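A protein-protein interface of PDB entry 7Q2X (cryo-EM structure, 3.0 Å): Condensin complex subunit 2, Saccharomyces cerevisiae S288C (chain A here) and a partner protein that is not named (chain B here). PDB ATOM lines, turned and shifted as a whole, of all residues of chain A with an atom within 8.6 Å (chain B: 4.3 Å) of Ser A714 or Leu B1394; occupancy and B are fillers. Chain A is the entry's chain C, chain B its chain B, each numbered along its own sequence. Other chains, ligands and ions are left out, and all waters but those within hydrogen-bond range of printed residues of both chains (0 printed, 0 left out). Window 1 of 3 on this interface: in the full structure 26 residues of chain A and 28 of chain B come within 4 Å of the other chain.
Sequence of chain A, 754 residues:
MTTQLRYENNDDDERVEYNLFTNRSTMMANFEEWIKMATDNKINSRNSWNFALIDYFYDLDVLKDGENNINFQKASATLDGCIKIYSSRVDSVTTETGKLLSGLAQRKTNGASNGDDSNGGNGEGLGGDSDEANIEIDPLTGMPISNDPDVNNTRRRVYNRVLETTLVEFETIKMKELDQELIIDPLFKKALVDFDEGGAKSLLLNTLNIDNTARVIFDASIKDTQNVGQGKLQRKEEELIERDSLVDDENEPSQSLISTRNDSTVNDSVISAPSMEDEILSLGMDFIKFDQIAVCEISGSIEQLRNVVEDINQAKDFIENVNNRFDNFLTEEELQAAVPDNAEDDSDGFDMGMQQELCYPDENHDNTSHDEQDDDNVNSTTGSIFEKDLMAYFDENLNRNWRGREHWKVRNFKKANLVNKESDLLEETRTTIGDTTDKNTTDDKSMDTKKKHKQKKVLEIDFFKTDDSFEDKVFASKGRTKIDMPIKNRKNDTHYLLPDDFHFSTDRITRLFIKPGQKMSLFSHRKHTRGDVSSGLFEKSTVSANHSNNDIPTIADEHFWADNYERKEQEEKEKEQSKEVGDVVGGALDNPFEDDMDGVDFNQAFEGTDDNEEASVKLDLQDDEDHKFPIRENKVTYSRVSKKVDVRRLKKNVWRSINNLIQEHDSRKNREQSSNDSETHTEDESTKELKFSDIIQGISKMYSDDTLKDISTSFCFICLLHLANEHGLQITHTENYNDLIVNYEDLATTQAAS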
ATOM      1  N   VAL A 645      18.508 -24.008   9.177  1.00  0.00           N
ATOM      2  CA  VAL A 645      17.522 -24.693   8.360  1.00  0.00           C
ATOM      3  C   VAL A 645      18.125 -25.821   7.528  1.00  0.00           C
ATOM      4  O   VAL A 645      17.489 -26.873   7.388  1.00  0.00           O
ATOM      5  CB  VAL A 645      16.780 -23.685   7.455  1.00  0.00           C
ATOM      6  CG1 VAL A 645      15.809 -24.399   6.526  1.00  0.00           C
ATOM      7  CG2 VAL A 645      16.053 -22.649   8.301  1.00  0.00           C
ATOM      8  N   VAL A 647      18.860 -25.790   4.097  1.00  0.00           N
ATOM      9  CA  VAL A 647      17.884 -25.780   3.011  1.00  0.00           C
ATOM     10  C   VAL A 647      18.155 -26.894   2.007  1.00  0.00           C
ATOM     11  O   VAL A 647      17.216 -27.479   1.455  1.00  0.00           O
ATOM     12  CB  VAL A 647      17.873 -24.398   2.328  1.00  0.00           C
ATOM     13  CG1 VAL A 647      16.740 -24.308   1.317  1.00  0.00           C
ATOM     14  CG2 VAL A 647      17.757 -23.295   3.370  1.00  0.00           C
ATOM     15  N   LEU A 650      16.749 -30.150   3.454  1.00  0.00           N
ATOM     16  CA  LEU A 650      15.291 -30.144   3.415  1.00  0.00           C
ATOM     17  C   LEU A 650      14.785 -30.347   1.993  1.00  0.00           C
ATOM     18  O   LEU A 650      13.809 -31.070   1.772  1.00  0.00           O
ATOM     19  CB  LEU A 650      14.759 -28.835   4.003  1.00  0.00           C
ATOM     20  CG  LEU A 650      13.266 -28.713   4.326  1.00  0.00           C
ATOM     21  CD1 LEU A 650      13.072 -27.708   5.447  1.00  0.00           C
ATOM     22  CD2 LEU A 650      12.432 -28.315   3.118  1.00  0.00           C
ATOM     23  N   PHE A 692       0.082 -31.250  -1.311  1.00  0.00           N
ATOM     24  CA  PHE A 692       1.214 -30.696  -0.573  1.00  0.00           C
ATOM     25  C   PHE A 692       1.241 -31.173   0.876  1.00  0.00           C
ATOM     26  O   PHE A 692       2.323 -31.333   1.456  1.00  0.00           O
ATOM     27  CB  PHE A 692       1.170 -29.168  -0.633  1.00  0.00           C
ATOM     28  CG  PHE A 692       2.441 -28.501  -0.187  1.00  0.00           C
ATOM     29  CD1 PHE A 692       3.674 -28.960  -0.618  1.00  0.00           C
ATOM     30  CD2 PHE A 692       2.400 -27.402   0.657  1.00  0.00           C
ATOM     31  CE1 PHE A 692       4.842 -28.343  -0.211  1.00  0.00           C
ATOM     32  CE2 PHE A 692       3.565 -26.781   1.067  1.00  0.00           C
ATOM     33  CZ  PHE A 692       4.787 -27.252   0.633  1.00  0.00           C
ATOM     34  N   ILE A 696       4.274 -32.625   3.229  1.00  0.00           N
ATOM     35  CA  ILE A 696       4.641 -32.139   4.557  1.00  0.00           C
ATOM     36  C   ILE A 696       4.725 -33.297   5.540  1.00  0.00           C
ATOM     37  O   ILE A 696       5.690 -33.415   6.307  1.00  0.00           O
ATOM     38  CB  ILE A 696       3.637 -31.071   5.032  1.00  0.00           C
ATOM     39  CG1 ILE A 696       3.649 -29.863   4.092  1.00  0.00           C
ATOM     40  CG2 ILE A 696       3.951 -30.641   6.457  1.00  0.00           C
ATOM     41  CD1 ILE A 696       5.030 -29.343   3.784  1.00  0.00           C
ATOM     42  N   ASP A 710      11.566 -25.932  14.252  1.00  0.00           N
ATOM     43  CA  ASP A 710      12.275 -24.905  13.500  1.00  0.00           C
ATOM     44  C   ASP A 710      11.738 -24.750  12.081  1.00  0.00           C
ATOM     45  O   ASP A 710      11.685 -23.631  11.560  1.00  0.00           O
ATOM     46  CB  ASP A 710      13.772 -25.222  13.456  1.00  0.00           C
ATOM     47  CG  ASP A 710      14.540 -24.573  14.591  1.00  0.00           C
ATOM     48  OD1 ASP A 710      13.900 -23.955  15.467  1.00  0.00           O
ATOM     49  OD2 ASP A 710      15.785 -24.678  14.607  1.00  0.00           O
ATOM     50  N   ILE A 711      11.335 -25.851  11.445  1.00  0.00           N
ATOM     51  CA  ILE A 711      10.880 -25.796  10.060  1.00  0.00           C
ATOM     52  C   ILE A 711       9.428 -25.344  10.008  1.00  0.00           C
ATOM     53  O   ILE A 711       8.571 -25.854  10.742  1.00  0.00           O
ATOM     54  CB  ILE A 711      11.059 -27.158   9.375  1.00  0.00           C
ATOM     55  CG1 ILE A 711      12.537 -27.539   9.310  1.00  0.00           C
ATOM     56  CG2 ILE A 711      10.447 -27.145   7.983  1.00  0.00           C
ATOM     57  CD1 ILE A 711      12.769 -28.967   8.885  1.00  0.00           C
ATOM     58  N   SER A 712       9.145 -24.382   9.134  1.00  0.00           N
ATOM     59  CA  SER A 712       7.795 -23.912   8.866  1.00  0.00           C
ATOM     60  C   SER A 712       7.420 -24.232   7.424  1.00  0.00           C
ATOM     61  O   SER A 712       8.210 -24.792   6.660  1.00  0.00           O
ATOM     62  CB  SER A 712       7.668 -22.407   9.133  1.00  0.00           C
ATOM     63  OG  SER A 712       8.451 -21.659   8.219  1.00  0.00           O
ATOM     64  N   THR A 713       6.189 -23.869   7.056  1.00  0.00           N
ATOM     65  CA  THR A 713       5.707 -24.129   5.704  1.00  0.00           C
ATOM     66  C   THR A 713       6.426 -23.286   4.658  1.00  0.00           C
ATOM     67  O   THR A 713       6.453 -23.670   3.483  1.00  0.00           O
ATOM     68  CB  THR A 713       4.199 -23.880   5.622  1.00  0.00           C
ATOM     69  OG1 THR A 713       3.742 -24.126   4.286  1.00  0.00           O
ATOM     70  CG2 THR A 713       3.870 -22.447   6.012  1.00  0.00           C
ATOM     71  N   SER A 714       7.010 -22.154   5.059  1.00  0.00           N
ATOM     72  CA  SER A 714       7.704 -21.296   4.105  1.00  0.00           C
ATOM     73  C   SER A 714       8.922 -21.994   3.514  1.00  0.00           C
ATOM     74  O   SER A 714       9.207 -21.855   2.318  1.00  0.00           O
ATOM     75  CB  SER A 714       8.114 -19.989   4.782  1.00  0.00           C
ATOM     76  OG  SER A 714       6.997 -19.329   5.348  1.00  0.00           O
ATOM     77  N   PHE A 715       9.659 -22.742   4.339  1.00  0.00           N
ATOM     78  CA  PHE A 715      10.829 -23.465   3.851  1.00  0.00           C
ATOM     79  C   PHE A 715      10.430 -24.491   2.802  1.00  0.00           C
ATOM     80  O   PHE A 715      11.062 -24.602   1.744  1.00  0.00           O
ATOM     81  CB  PHE A 715      11.539 -24.156   5.015  1.00  0.00           C
ATOM     82  CG  PHE A 715      11.908 -23.233   6.139  1.00  0.00           C
ATOM     83  CD1 PHE A 715      12.164 -21.893   5.906  1.00  0.00           C
ATOM     84  CD2 PHE A 715      11.977 -23.707   7.440  1.00  0.00           C
ATOM     85  CE1 PHE A 715      12.499 -21.047   6.946  1.00  0.00           C
ATOM     86  CE2 PHE A 715      12.308 -22.866   8.482  1.00  0.00           C
ATOM     87  CZ  PHE A 715      12.567 -21.536   8.233  1.00  0.00           C
ATOM     88  N   CYS A 716       9.372 -25.254   3.086  1.00  0.00           N
ATOM     89  CA  CYS A 716       8.892 -26.248   2.135  1.00  0.00           C
ATOM     90  C   CYS A 716       8.404 -25.585   0.856  1.00  0.00           C
ATOM     91  O   CYS A 716       8.627 -26.104  -0.243  1.00  0.00           O
ATOM     92  CB  CYS A 716       7.781 -27.081   2.771  1.00  0.00           C
ATOM     93  SG  CYS A 716       8.170 -27.669   4.431  1.00  0.00           S
ATOM     94  N   PHE A 717       7.738 -24.435   0.982  1.00  0.00           N
ATOM     95  CA  PHE A 717       7.281 -23.705  -0.196  1.00  0.00           C
ATOM     96  C   PHE A 717       8.460 -23.275  -1.065  1.00  0.00           C
ATOM     97  O   PHE A 717       8.451 -23.468  -2.286  1.00  0.00           O
ATOM     98  CB  PHE A 717       6.459 -22.493   0.243  1.00  0.00           C
ATOM     99  CG  PHE A 717       5.679 -21.848  -0.865  1.00  0.00           C
ATOM    100  CD1 PHE A 717       5.009 -22.619  -1.797  1.00  0.00           C
ATOM    101  CD2 PHE A 717       5.615 -20.469  -0.970  1.00  0.00           C
ATOM    102  CE1 PHE A 717       4.285 -22.026  -2.814  1.00  0.00           C
ATOM    103  CE2 PHE A 717       4.897 -19.871  -1.986  1.00  0.00           C
ATOM    104  CZ  PHE A 717       4.231 -20.650  -2.909  1.00  0.00           C
ATOM    105  N   ILE A 718       9.495 -22.706  -0.442  1.00  0.00           N
ATOM    106  CA  ILE A 718      10.659 -22.246  -1.193  1.00  0.00           C
ATOM    107  C   ILE A 718      11.367 -23.421  -1.856  1.00  0.00           C
ATOM    108  O   ILE A 718      11.814 -23.327  -3.007  1.00  0.00           O
ATOM    109  CB  ILE A 718      11.607 -21.454  -0.273  1.00  0.00           C
ATOM    110  CG1 ILE A 718      10.942 -20.155   0.183  1.00  0.00           C
ATOM    111  CG2 ILE A 718      12.923 -21.159  -0.975  1.00  0.00           C
ATOM    112  CD1 ILE A 718      11.716 -19.420   1.248  1.00  0.00           C
ATOM    113  N   CYS A 719      11.479 -24.546  -1.147  1.00  0.00           N
ATOM    114  CA  CYS A 719      12.102 -25.725  -1.740  1.00  0.00           C
ATOM    115  C   CYS A 719      11.270 -26.269  -2.896  1.00  0.00           C
ATOM    116  O   CYS A 719      11.822 -26.772  -3.882  1.00  0.00           O
ATOM    117  CB  CYS A 719      12.317 -26.795  -0.672  1.00  0.00           C
ATOM    118  SG  CYS A 719      13.749 -26.483   0.387  1.00  0.00           S
ATOM    119  N   LEU A 720       9.942 -26.178  -2.796  1.00  0.00           N
ATOM    120  CA  LEU A 720       9.087 -26.621  -3.892  1.00  0.00           C
ATOM    121  C   LEU A 720       9.256 -25.728  -5.116  1.00  0.00           C
ATOM    122  O   LEU A 720       9.298 -26.219  -6.252  1.00  0.00           O
ATOM    123  CB  LEU A 720       7.629 -26.655  -3.430  1.00  0.00           C
ATOM    124  CG  LEU A 720       6.624 -27.393  -4.315  1.00  0.00           C
ATOM    125  CD1 LEU A 720       6.598 -28.869  -3.960  1.00  0.00           C
ATOM    126  CD2 LEU A 720       5.243 -26.790  -4.147  1.00  0.00           C
ATOM    127  N   LEU A 721       9.363 -24.412  -4.907  1.00  0.00           N
ATOM    128  CA  LEU A 721       9.688 -23.518  -6.018  1.00  0.00           C
ATOM    129  C   LEU A 721      11.052 -23.837  -6.620  1.00  0.00           C
ATOM    130  O   LEU A 721      11.218 -23.791  -7.842  1.00  0.00           O
ATOM    131  CB  LEU A 721       9.631 -22.051  -5.588  1.00  0.00           C
ATOM    132  CG  LEU A 721       8.296 -21.301  -5.542  1.00  0.00           C
ATOM    133  CD1 LEU A 721       7.373 -21.728  -4.428  1.00  0.00           C
ATOM    134  CD2 LEU A 721       8.587 -19.816  -5.441  1.00  0.00           C
ATOM    135  N   HIS A 722      12.044 -24.145  -5.783  1.00  0.00           N
ATOM    136  CA  HIS A 722      13.359 -24.503  -6.314  1.00  0.00           C
ATOM    137  C   HIS A 722      13.289 -25.775  -7.154  1.00  0.00           C
ATOM    138  O   HIS A 722      13.891 -25.854  -8.235  1.00  0.00           O
ATOM    139  CB  HIS A 722      14.363 -24.668  -5.173  1.00  0.00           C
ATOM    140  CG  HIS A 722      15.011 -23.385  -4.750  1.00  0.00           C
ATOM    141  ND1 HIS A 722      14.458 -22.546  -3.807  1.00  0.00           N
ATOM    142  CD2 HIS A 722      16.166 -22.798  -5.145  1.00  0.00           C
ATOM    143  CE1 HIS A 722      15.245 -21.498  -3.637  1.00  0.00           C
ATOM    144  NE2 HIS A 722      16.288 -21.627  -4.437  1.00  0.00           N
ATOM    145  N   TYR A 737      -7.573 -21.065  -1.548  1.00  0.00           N
ATOM    146  CA  TYR A 737      -6.232 -20.516  -1.322  1.00  0.00           C
ATOM    147  C   TYR A 737      -5.655 -20.973   0.015  1.00  0.00           C
ATOM    148  O   TYR A 737      -4.951 -20.223   0.696  1.00  0.00           O
ATOM    149  CB  TYR A 737      -6.232 -18.987  -1.417  1.00  0.00           C
ATOM    150  CG  TYR A 737      -6.427 -18.455  -2.817  1.00  0.00           C
ATOM    151  CD1 TYR A 737      -5.439 -18.609  -3.781  1.00  0.00           C
ATOM    152  CD2 TYR A 737      -7.597 -17.801  -3.176  1.00  0.00           C
ATOM    153  CE1 TYR A 737      -5.611 -18.123  -5.063  1.00  0.00           C
ATOM    154  CE2 TYR A 737      -7.778 -17.313  -4.455  1.00  0.00           C
ATOM    155  CZ  TYR A 737      -6.782 -17.476  -5.394  1.00  0.00           C
ATOM    156  OH  TYR A 737      -6.961 -16.990  -6.669  1.00  0.00           O
ATOM    157  N   LEU A 740      -2.185 -26.265  -1.797  1.00  0.00           N
ATOM    158  CA  LEU A 740      -1.681 -26.258  -3.162  1.00  0.00           C
ATOM    159  C   LEU A 740      -1.564 -27.678  -3.697  1.00  0.00           C
ATOM    160  O   LEU A 740      -1.192 -28.600  -2.964  1.00  0.00           O
ATOM    161  CB  LEU A 740      -0.320 -25.559  -3.234  1.00  0.00           C
ATOM    162  CG  LEU A 740      -0.292 -24.031  -3.201  1.00  0.00           C
ATOM    163  CD1 LEU A 740      -0.650 -23.520  -1.821  1.00  0.00           C
ATOM    164  CD2 LEU A 740       1.088 -23.540  -3.593  1.00  0.00           C
ATOM    165  N   ALA B 182       4.223 -11.167   1.324  1.00  0.00           N
ATOM    166  CA  ALA B 182       5.621 -11.422   1.012  1.00  0.00           C
ATOM    167  C   ALA B 182       5.731 -12.195  -0.293  1.00  0.00           C
ATOM    168  O   ALA B 182       4.979 -13.146  -0.529  1.00  0.00           O
ATOM    169  CB  ALA B 182       6.308 -12.200   2.138  1.00  0.00           C
ATOM    170  N   PHE B1388       9.977 -13.642   5.914  1.00  0.00           N
ATOM    171  CA  PHE B1388       8.866 -14.450   5.428  1.00  0.00           C
ATOM    172  C   PHE B1388       8.372 -15.493   6.421  1.00  0.00           C
ATOM    173  O   PHE B1388       7.393 -16.182   6.116  1.00  0.00           O
ATOM    174  CB  PHE B1388       9.209 -15.121   4.083  1.00  0.00           C
ATOM    175  CG  PHE B1388      10.429 -15.992   4.109  1.00  0.00           C
ATOM    176  CD1 PHE B1388      10.358 -17.295   4.582  1.00  0.00           C
ATOM    177  CD2 PHE B1388      11.638 -15.524   3.638  1.00  0.00           C
ATOM    178  CE1 PHE B1388      11.481 -18.098   4.599  1.00  0.00           C
ATOM    179  CE2 PHE B1388      12.762 -16.324   3.649  1.00  0.00           C
ATOM    180  CZ  PHE B1388      12.684 -17.612   4.132  1.00  0.00           C
ATOM    181  N   ALA B1391       4.968 -13.490   7.572  1.00  0.00           N
ATOM    182  CA  ALA B1391       3.950 -13.115   6.604  1.00  0.00           C
ATOM    183  C   ALA B1391       2.732 -14.028   6.724  1.00  0.00           C
ATOM    184  O   ALA B1391       2.809 -15.144   7.244  1.00  0.00           O
ATOM    185  CB  ALA B1391       4.507 -13.173   5.183  1.00  0.00           C
ATOM    186  N   GLN B1393       0.653 -14.412   3.763  1.00  0.00           N
ATOM    187  CA  GLN B1393       0.356 -14.908   2.424  1.00  0.00           C
ATOM    188  C   GLN B1393       1.592 -14.724   1.563  1.00  0.00           C
ATOM    189  O   GLN B1393       2.073 -13.597   1.403  1.00  0.00           O
ATOM    190  CB  GLN B1393      -0.841 -14.163   1.837  1.00  0.00           C
ATOM    191  CG  GLN B1393      -1.294 -14.641   0.474  1.00  0.00           C
ATOM    192  CD  GLN B1393      -2.685 -14.147   0.136  1.00  0.00           C
ATOM    193  OE1 GLN B1393      -3.291 -14.576  -0.845  1.00  0.00           O
ATOM    194  NE2 GLN B1393      -3.203 -13.240   0.955  1.00  0.00           N
ATOM    195  N   LEU B1394       2.106 -15.820   1.015  1.00  0.00           N
ATOM    196  CA  LEU B1394       3.296 -15.789   0.177  1.00  0.00           C
ATOM    197  C   LEU B1394       2.917 -15.969  -1.286  1.00  0.00           C
ATOM    198  O   LEU B1394       2.121 -16.850  -1.628  1.00  0.00           O
ATOM    199  CB  LEU B1394       4.300 -16.864   0.595  1.00  0.00           C
ATOM    200  CG  LEU B1394       4.459 -17.115   2.093  1.00  0.00           C
ATOM    201  CD1 LEU B1394       5.294 -18.360   2.351  1.00  0.00           C
ATOM    202  CD2 LEU B1394       5.079 -15.905   2.769  1.00  0.00           C
ATOM    203  N   VAL B1395       3.478 -15.118  -2.137  1.00  0.00           N
ATOM    204  CA  VAL B1395       3.357 -15.235  -3.583  1.00  0.00           C
ATOM    205  C   VAL B1395       4.710 -15.701  -4.101  1.00  0.00           C
ATOM    206  O   VAL B1395       5.720 -15.005  -3.938  1.00  0.00           O
ATOM    207  CB  VAL B1395       2.934 -13.911  -4.231  1.00  0.00           C
ATOM    208  CG1 VAL B1395       2.916 -14.041  -5.745  1.00  0.00           C
ATOM    209  CG2 VAL B1395       1.572 -13.481  -3.711  1.00  0.00           C
ATOM    210  N   GLY B1396       4.741 -16.880  -4.713  1.00  0.00           N
ATOM    211  CA  GLY B1396       5.969 -17.465  -5.216  1.00  0.00           C
ATOM    212  C   GLY B1396       5.975 -17.514  -6.732  1.00  0.00           C
ATOM    213  O   GLY B1396       4.922 -17.610  -7.365  1.00  0.00           O
ATOM    214  N   THR B1407       2.265 -18.548  -8.014  1.00  0.00           N
ATOM    215  CA  THR B1407       1.311 -19.276  -7.189  1.00  0.00           C
ATOM    216  C   THR B1407       1.215 -18.579  -5.837  1.00  0.00           C
ATOM    217  O   THR B1407       2.105 -17.816  -5.454  1.00  0.00           O
ATOM    218  CB  THR B1407       1.720 -20.749  -7.022  1.00  0.00           C
ATOM    219  OG1 THR B1407       2.103 -21.283  -8.295  1.00  0.00           O
ATOM    220  CG2 THR B1407       0.553 -21.574  -6.507  1.00  0.00           C
ATOM    221  N   THR B1408       0.119 -18.830  -5.122  1.00  0.00           N
ATOM    222  CA  THR B1408      -0.183 -18.132  -3.879  1.00  0.00           C
ATOM    223  C   THR B1408      -0.493 -19.135  -2.777  1.00  0.00           C
ATOM    224  O   THR B1408      -1.214 -20.111  -3.011  1.00  0.00           O
ATOM    225  CB  THR B1408      -1.365 -17.176  -4.076  1.00  0.00           C
ATOM    226  OG1 THR B1408      -1.034 -16.212  -5.083  1.00  0.00           O
ATOM    227  CG2 THR B1408      -1.698 -16.458  -2.783  1.00  0.00           C
ATOM    228  N   ILE B1409       0.036 -18.890  -1.576  1.00  0.00           N
ATOM    229  CA  ILE B1409      -0.180 -19.759  -0.422  1.00  0.00           C
ATOM    230  C   ILE B1409      -0.534 -18.901   0.788  1.00  0.00           C
ATOM    231  O   ILE B1409      -0.009 -17.795   0.949  1.00  0.00           O
ATOM    232  CB  ILE B1409       1.054 -20.638  -0.121  1.00  0.00           C
ATOM    233  CG1 ILE B1409       0.718 -21.710   0.919  1.00  0.00           C
ATOM    234  CG2 ILE B1409       2.227 -19.796   0.353  1.00  0.00           C
ATOM    235  CD1 ILE B1409       1.762 -22.804   1.034  1.00  0.00           C
ATOM    236  N   ASN B1411      -0.444 -18.638   4.938  1.00  0.00           N
ATOM    237  CA  ASN B1411       0.465 -19.135   5.970  1.00  0.00           C
ATOM    238  C   ASN B1411      -0.333 -19.821   7.071  1.00  0.00           C
ATOM    239  O   ASN B1411      -1.023 -19.169   7.859  1.00  0.00           O
ATOM    240  CB  ASN B1411       1.306 -17.999   6.536  1.00  0.00           C
ATOM    241  CG  ASN B1411       2.518 -17.698   5.686  1.00  0.00           C
ATOM    242  OD1 ASN B1411       2.494 -17.876   4.470  1.00  0.00           O
ATOM    243  ND2 ASN B1411       3.591 -17.242   6.321  1.00  0.00           N
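The side-chain sulfur of Cys A719 lies close to the backbone carbonyl oxygen of Phe A715, at 3.5 Å. N of Phe A692 sits close to O of Leu A740, 3.4 Å away. The backbone NH of Leu B1394 lies within hydrogen-bond range of the backbone carbonyl oxygen of Ile B1409 (2.9 Å). The backbone carbonyl oxygen (O) of Ile A718 sits at hydrogen-bond distance from a ring nitrogen (ND1) of His A722, 2.9 Å away. The backbone NH of Thr B1407 is in hydrogen-bond range of the backbone carbonyl oxygen of Gly B1396 (2.9 Å).
Among the printed residues, pairs that only touch across the chains: Ser A714 with Leu B1394 (3.6 Å), Phe A715 with Phe B1388 (3.9 Å), Phe A717 with Leu B1394 (3.9 Å), Phe A717 with Ile B1409 (3.6 Å), Ile A718 with Phe B1388 (3.5 Å), Leu A721 with Gly B1396 (3.5 Å), Leu A740 with Thr B1407 (3.6 Å), Leu A740 with Thr B1408 (3.7 Å) and Leu A740 with Ile B1409 (3.6 Å).
Ser A714 touches just these residues of chain B: Phe B1388 (3.3 Å) and Leu B1394 (3.6 Å). Of chain A, only Ser A714 (3.6 Å) and Phe A717 (3.9 Å) come within 4 Å of Leu B1394. Printed residues of chain B within 4 Å of Phe A715: Phe B1388. Of the printed residues of chain A, Ile B1409 touches Phe A717 and Leu A740. Of the printed residues of chain B, Leu A721 touches Gly B1396 (3.5 Å). Of the printed residues of chain B, Leu A740 touches Thr B1407, Thr B1408 and Ile B1409. Printed residues of chain A within 4 Å of Thr B1408: Leu A740 (3.7 Å). Ser A712 touches none of the printed residues of chain B. The nearest residue of chain A that does not touch Leu B1394 is Thr A713 (5.6 Å).
The backbone carbonyl oxygen (O) of Phe B1388 is in hydrogen-bond range of the side-chain hydroxyl (OG) of Ser A714.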
